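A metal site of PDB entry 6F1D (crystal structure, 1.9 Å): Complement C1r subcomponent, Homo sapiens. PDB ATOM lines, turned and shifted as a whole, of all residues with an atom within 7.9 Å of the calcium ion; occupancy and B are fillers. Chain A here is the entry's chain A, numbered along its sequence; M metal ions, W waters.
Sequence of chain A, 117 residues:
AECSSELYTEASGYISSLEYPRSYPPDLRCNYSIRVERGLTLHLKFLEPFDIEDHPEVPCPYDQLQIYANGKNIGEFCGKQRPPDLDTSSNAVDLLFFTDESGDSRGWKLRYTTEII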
ATOM      1  N   TYR A  24     -20.861 -23.486  16.667  1.00  0.00           N
ATOM      2  CA  TYR A  24     -20.698 -22.056  16.967  1.00  0.00           C
ATOM      3  C   TYR A  24     -21.965 -21.467  17.585  1.00  0.00           C
ATOM      4  O   TYR A  24     -23.078 -21.965  17.383  1.00  0.00           O
ATOM      5  CB  TYR A  24     -20.262 -21.282  15.743  1.00  0.00           C
ATOM      6  CG  TYR A  24     -21.113 -21.503  14.524  1.00  0.00           C
ATOM      7  CD1 TYR A  24     -22.316 -20.841  14.387  1.00  0.00           C
ATOM      8  CD2 TYR A  24     -20.690 -22.372  13.522  1.00  0.00           C
ATOM      9  CE1 TYR A  24     -23.118 -21.025  13.277  1.00  0.00           C
ATOM     10  CE2 TYR A  24     -21.479 -22.574  12.373  1.00  0.00           C
ATOM     11  CZ  TYR A  24     -22.702 -21.892  12.282  1.00  0.00           C
ATOM     12  OH  TYR A  24     -23.493 -22.019  11.163  1.00  0.00           O
ATOM     13  N   PRO A  25     -21.826 -20.448  18.415  1.00  0.00           N
ATOM     14  CA  PRO A  25     -22.984 -19.853  19.126  1.00  0.00           C
ATOM     15  C   PRO A  25     -23.901 -19.100  18.173  1.00  0.00           C
ATOM     16  O   PRO A  25     -23.482 -18.683  17.092  1.00  0.00           O
ATOM     17  CB  PRO A  25     -22.329 -18.880  20.121  1.00  0.00           C
ATOM     18  CG  PRO A  25     -20.863 -19.123  20.020  1.00  0.00           C
ATOM     19  CD  PRO A  25     -20.590 -19.729  18.711  1.00  0.00           C
ATOM     20  N   PRO A  26     -25.152 -18.833  18.565  1.00  0.00           N
ATOM     21  CA  PRO A  26     -26.046 -18.063  17.716  1.00  0.00           C
ATOM     22  C   PRO A  26     -25.884 -16.553  17.931  1.00  0.00           C
ATOM     23  O   PRO A  26     -25.200 -16.101  18.837  1.00  0.00           O
ATOM     24  CB  PRO A  26     -27.437 -18.527  18.195  1.00  0.00           C
ATOM     25  CG  PRO A  26     -27.241 -18.757  19.650  1.00  0.00           C
ATOM     26  CD  PRO A  26     -25.837 -19.285  19.798  1.00  0.00           C
ATOM     27  N   ASP A  27     -26.509 -15.792  17.019  1.00  0.00           N
ATOM     28  CA  ASP A  27     -26.654 -14.347  17.095  1.00  0.00           C
ATOM     29  C   ASP A  27     -25.312 -13.623  17.104  1.00  0.00           C
ATOM     30  O   ASP A  27     -25.190 -12.540  17.679  1.00  0.00           O
ATOM     31  CB  ASP A  27     -27.523 -13.954  18.288  1.00  0.00           C
ATOM     32  CG  ASP A  27     -28.930 -14.502  18.158  1.00  0.00           C
ATOM     33  OD1 ASP A  27     -29.528 -14.356  17.054  1.00  0.00           O
ATOM     34  OD2 ASP A  27     -29.450 -15.110  19.128  1.00  0.00           O
ATOM     35  N   ILE A  52     -21.254 -24.629   7.791  1.00  0.00           N
ATOM     36  CA  ILE A  52     -22.040 -23.437   8.139  1.00  0.00           C
ATOM     37  C   ILE A  52     -23.447 -23.734   7.665  1.00  0.00           C
ATOM     38  O   ILE A  52     -23.636 -24.188   6.528  1.00  0.00           O
ATOM     39  CB  ILE A  52     -21.477 -22.172   7.473  1.00  0.00           C
ATOM     40  CG1 ILE A  52     -20.034 -21.912   7.950  1.00  0.00           C
ATOM     41  CG2 ILE A  52     -22.406 -20.929   7.721  1.00  0.00           C
ATOM     42  CD1 ILE A  52     -19.410 -20.672   7.338  1.00  0.00           C
ATOM     43  N   GLU A  53     -24.429 -23.478   8.531  1.00  0.00           N
ATOM     44  CA  GLU A  53     -25.798 -23.889   8.235  1.00  0.00           C
ATOM     45  C   GLU A  53     -26.255 -23.270   6.914  1.00  0.00           C
ATOM     46  O   GLU A  53     -25.968 -22.086   6.637  1.00  0.00           O
ATOM     47  CB  GLU A  53     -26.691 -23.449   9.417  1.00  0.00           C
ATOM     48  CG  GLU A  53     -28.205 -23.797   9.274  1.00  0.00           C
ATOM     49  CD  GLU A  53     -29.056 -23.155  10.359  1.00  0.00           C
ATOM     50  OE1 GLU A  53     -30.189 -23.623  10.619  1.00  0.00           O
ATOM     51  OE2 GLU A  53     -28.617 -22.140  10.953  1.00  0.00           O
ATOM     52  N   ASP A  54     -26.919 -24.059   6.066  1.00  0.00           N
ATOM     53  CA  ASP A  54     -27.354 -23.555   4.761  1.00  0.00           C
ATOM     54  C   ASP A  54     -28.826 -23.883   4.509  1.00  0.00           C
ATOM     55  O   ASP A  54     -29.567 -24.304   5.401  1.00  0.00           O
ATOM     56  CB  ASP A  54     -26.500 -24.095   3.603  1.00  0.00           C
ATOM     57  CG  ASP A  54     -26.633 -25.581   3.422  1.00  0.00           C
ATOM     58  OD1 ASP A  54     -27.303 -26.231   4.272  1.00  0.00           O
ATOM     59  OD2 ASP A  54     -26.069 -26.126   2.440  1.00  0.00           O
ATOM     60  N   TYR A  62     -29.224 -18.122   6.404  1.00  0.00           N
ATOM     61  CA  TYR A  62     -29.243 -18.271   7.865  1.00  0.00           C
ATOM     62  C   TYR A  62     -27.991 -17.657   8.470  1.00  0.00           C
ATOM     63  O   TYR A  62     -28.050 -16.655   9.183  1.00  0.00           O
ATOM     64  CB  TYR A  62     -29.341 -19.751   8.224  1.00  0.00           C
ATOM     65  CG  TYR A  62     -30.650 -20.413   7.808  1.00  0.00           C
ATOM     66  CD1 TYR A  62     -30.648 -21.639   7.157  1.00  0.00           C
ATOM     67  CD2 TYR A  62     -31.881 -19.806   8.067  1.00  0.00           C
ATOM     68  CE1 TYR A  62     -31.812 -22.245   6.781  1.00  0.00           C
ATOM     69  CE2 TYR A  62     -33.058 -20.415   7.692  1.00  0.00           C
ATOM     70  CZ  TYR A  62     -33.001 -21.648   7.069  1.00  0.00           C
ATOM     71  OH  TYR A  62     -34.171 -22.258   6.687  1.00  0.00           O
ATOM     72  N   ASP A  63     -26.854 -18.281   8.198  1.00  0.00           N
ATOM     73  CA  ASP A  63     -25.567 -17.874   8.732  1.00  0.00           C
ATOM     74  C   ASP A  63     -24.691 -17.594   7.528  1.00  0.00           C
ATOM     75  O   ASP A  63     -24.900 -18.213   6.483  1.00  0.00           O
ATOM     76  CB  ASP A  63     -24.887 -18.993   9.585  1.00  0.00           C
ATOM     77  CG  ASP A  63     -25.789 -19.523  10.686  1.00  0.00           C
ATOM     78  OD1 ASP A  63     -26.728 -18.830  11.104  1.00  0.00           O
ATOM     79  OD2 ASP A  63     -25.560 -20.677  11.118  1.00  0.00           O
ATOM     80  N   GLN A  64     -23.716 -16.677   7.660  1.00  0.00           N
ATOM     81  CA  GLN A  64     -22.891 -16.328   6.498  1.00  0.00           C
ATOM     82  C   GLN A  64     -21.474 -16.102   6.946  1.00  0.00           C
ATOM     83  O   GLN A  64     -21.254 -15.410   7.950  1.00  0.00           O
ATOM     84  CB  GLN A  64     -23.359 -15.039   5.799  1.00  0.00           C
ATOM     85  CG  GLN A  64     -24.809 -15.039   5.331  1.00  0.00           C
ATOM     86  CD  GLN A  64     -25.820 -14.702   6.460  1.00  0.00           C
ATOM     87  OE1 GLN A  64     -25.514 -13.940   7.366  1.00  0.00           O
ATOM     88  NE2 GLN A  64     -27.042 -15.230   6.332  1.00  0.00           N
ATOM     89  N   PHE A  97     -18.401 -13.010  10.179  1.00  0.00           N
ATOM     90  CA  PHE A  97     -19.216 -14.201  10.369  1.00  0.00           C
ATOM     91  C   PHE A  97     -20.504 -13.800  11.100  1.00  0.00           C
ATOM     92  O   PHE A  97     -20.437 -13.345  12.246  1.00  0.00           O
ATOM     93  CB  PHE A  97     -18.406 -15.224  11.174  1.00  0.00           C
ATOM     94  CG  PHE A  97     -19.052 -16.577  11.339  1.00  0.00           C
ATOM     95  CD1 PHE A  97     -18.962 -17.225  12.551  1.00  0.00           C
ATOM     96  CD2 PHE A  97     -19.686 -17.207  10.281  1.00  0.00           C
ATOM     97  CE1 PHE A  97     -19.547 -18.495  12.734  1.00  0.00           C
ATOM     98  CE2 PHE A  97     -20.262 -18.489  10.462  1.00  0.00           C
ATOM     99  CZ  PHE A  97     -20.169 -19.114  11.670  1.00  0.00           C
ATOM    100  N   PHE A  98     -21.650 -13.998  10.463  1.00  0.00           N
ATOM    101  CA  PHE A  98     -22.956 -13.681  11.031  1.00  0.00           C
ATOM    102  C   PHE A  98     -23.712 -14.972  11.268  1.00  0.00           C
ATOM    103  O   PHE A  98     -23.756 -15.828  10.378  1.00  0.00           O
ATOM    104  CB  PHE A  98     -23.801 -12.842  10.077  1.00  0.00           C
ATOM    105  CG  PHE A  98     -23.187 -11.519   9.703  1.00  0.00           C
ATOM    106  CD1 PHE A  98     -23.386 -10.399  10.497  1.00  0.00           C
ATOM    107  CD2 PHE A  98     -22.467 -11.377   8.505  1.00  0.00           C
ATOM    108  CE1 PHE A  98     -22.849  -9.163  10.147  1.00  0.00           C
ATOM    109  CE2 PHE A  98     -21.925 -10.134   8.144  1.00  0.00           C
ATOM    110  CZ  PHE A  98     -22.125  -9.031   8.971  1.00  0.00           C
ATOM    111  N   THR A  99     -24.326 -15.122  12.429  1.00  0.00           N
ATOM    112  CA  THR A  99     -25.112 -16.334  12.654  1.00  0.00           C
ATOM    113  C   THR A  99     -26.453 -15.942  13.221  1.00  0.00           C
ATOM    114  O   THR A  99     -26.593 -14.924  13.934  1.00  0.00           O
ATOM    115  CB  THR A  99     -24.422 -17.326  13.606  1.00  0.00           C
ATOM    116  OG1 THR A  99     -24.323 -16.739  14.913  1.00  0.00           O
ATOM    117  CG2 THR A  99     -22.996 -17.611  13.132  1.00  0.00           C
ATOM    118  N   ASP A 100     -27.447 -16.761  12.938  1.00  0.00           N
ATOM    119  CA  ASP A 100     -28.793 -16.429  13.360  1.00  0.00           C
ATOM    120  C   ASP A 100     -29.097 -17.099  14.694  1.00  0.00           C
ATOM    121  O   ASP A 100     -28.189 -17.540  15.392  1.00  0.00           O
ATOM    122  CB  ASP A 100     -29.807 -16.830  12.284  1.00  0.00           C
ATOM    123  CG  ASP A 100     -29.931 -18.365  12.115  1.00  0.00           C
ATOM    124  OD1 ASP A 100     -29.199 -19.146  12.778  1.00  0.00           O
ATOM    125  OD2 ASP A 100     -30.784 -18.786  11.291  1.00  0.00           O
ATOM    126  N   GLU A 101     -30.388 -17.268  15.031  1.00  0.00           N
ATOM    127  CA  GLU A 101     -30.767 -17.615  16.389  1.00  0.00           C
ATOM    128  C   GLU A 101     -30.670 -19.115  16.716  1.00  0.00           C
ATOM    129  O   GLU A 101     -30.818 -19.451  17.894  1.00  0.00           O
ATOM    130  CB  GLU A 101     -32.205 -17.127  16.668  1.00  0.00           C
ATOM    131  CG  GLU A 101     -33.281 -17.802  15.795  1.00  0.00           C
ATOM    132  CD  GLU A 101     -34.685 -17.200  15.969  1.00  0.00           C
ATOM    133  OE1 GLU A 101     -34.844 -15.946  15.877  1.00  0.00           O
ATOM    134  OE2 GLU A 101     -35.644 -17.975  16.212  1.00  0.00           O
ATOM    135  N   SER A 102     -30.462 -20.017  15.743  1.00  0.00           N
ATOM    136  CA  SER A 102     -30.551 -21.439  16.078  1.00  0.00           C
ATOM    137  C   SER A 102     -29.683 -22.292  15.151  1.00  0.00           C
ATOM    138  O   SER A 102     -29.174 -21.828  14.115  1.00  0.00           O
ATOM    139  CB  SER A 102     -31.993 -21.938  15.969  1.00  0.00           C
ATOM    140  OG  SER A 102     -32.361 -21.917  14.585  1.00  0.00           O
ATOM    141  N   GLY A 103     -29.549 -23.559  15.525  1.00  0.00           N
ATOM    142  CA  GLY A 103     -28.857 -24.580  14.767  1.00  0.00           C
ATOM    143  C   GLY A 103     -27.551 -25.004  15.434  1.00  0.00           C
ATOM    144  O   GLY A 103     -26.970 -24.290  16.267  1.00  0.00           O
ATOM    145  N   ASP A 104     -27.098 -26.204  15.063  1.00  0.00           N
ATOM    146  CA  ASP A 104     -25.871 -26.811  15.582  1.00  0.00           C
ATOM    147  C   ASP A 104     -25.036 -27.158  14.339  1.00  0.00           C
ATOM    148  O   ASP A 104     -25.317 -28.138  13.659  1.00  0.00           O
ATOM    149  CB  ASP A 104     -26.184 -28.057  16.388  1.00  0.00           C
ATOM    150  CG  ASP A 104     -26.655 -27.730  17.823  1.00  0.00           C
ATOM    151  OD1 ASP A 104     -25.902 -27.031  18.557  1.00  0.00           O
ATOM    152  OD2 ASP A 104     -27.756 -28.178  18.208  1.00  0.00           O
ATOM    153  N   SER A 105     -24.067 -26.321  14.014  1.00  0.00           N
ATOM    154  CA  SER A 105     -23.170 -26.546  12.881  1.00  0.00           C
ATOM    155  C   SER A 105     -21.754 -26.399  13.397  1.00  0.00           C
ATOM    156  O   SER A 105     -21.480 -25.579  14.296  1.00  0.00           O
ATOM    157  CB  SER A 105     -23.420 -25.559  11.716  1.00  0.00           C
ATOM    158  OG  SER A 105     -24.798 -25.256  11.596  1.00  0.00           O
HETATM  159 CA    CA M   1     -27.567 -20.824  12.546  1.00  0.00          CA
HETATM  160  O   HOH W   1     -26.631 -19.804  14.411  1.00  0.00           O
HETATM  161  O   HOH W   2     -26.185 -22.799  13.334  1.00  0.00           O
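The backbone NH of Glu 53 lies within hydrogen-bond range of the side-chain hydroxyl of Tyr 24, at 3.2 Å.
The backbone carbonyl oxygen (O) of Asp 100 is in hydrogen-bond range of the backbone NH (N) of Asp 27 (2.9 Å).
OD2 of Asp 63 lies close to OH of Tyr 24 (2.5 Å).
Of the 19 residues printed, 4 come within 4 Å of the calcium ion.
The nearest printed residue that does not touch the calcium ion is Tyr 24 (4.5 Å).
The calcium ion is bound by OE2 of Glu 53 (2.3 Å), water W1 (2.3 Å), OD1 of Asp 100 (2.4 Å), O of Ser 102 (2.5 Å), OD2 of Asp 63 (2.5 Å), water W2 (2.5 Å) and OD1 of Asp 63 (2.6 Å).
The calcium ion has seven donor atoms within binding distance.
Water W2 lies within hydrogen-bond range of the side-chain hydroxyl (OG) of Ser 105 and the backbone carbonyl oxygen (O) of Gly 103.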
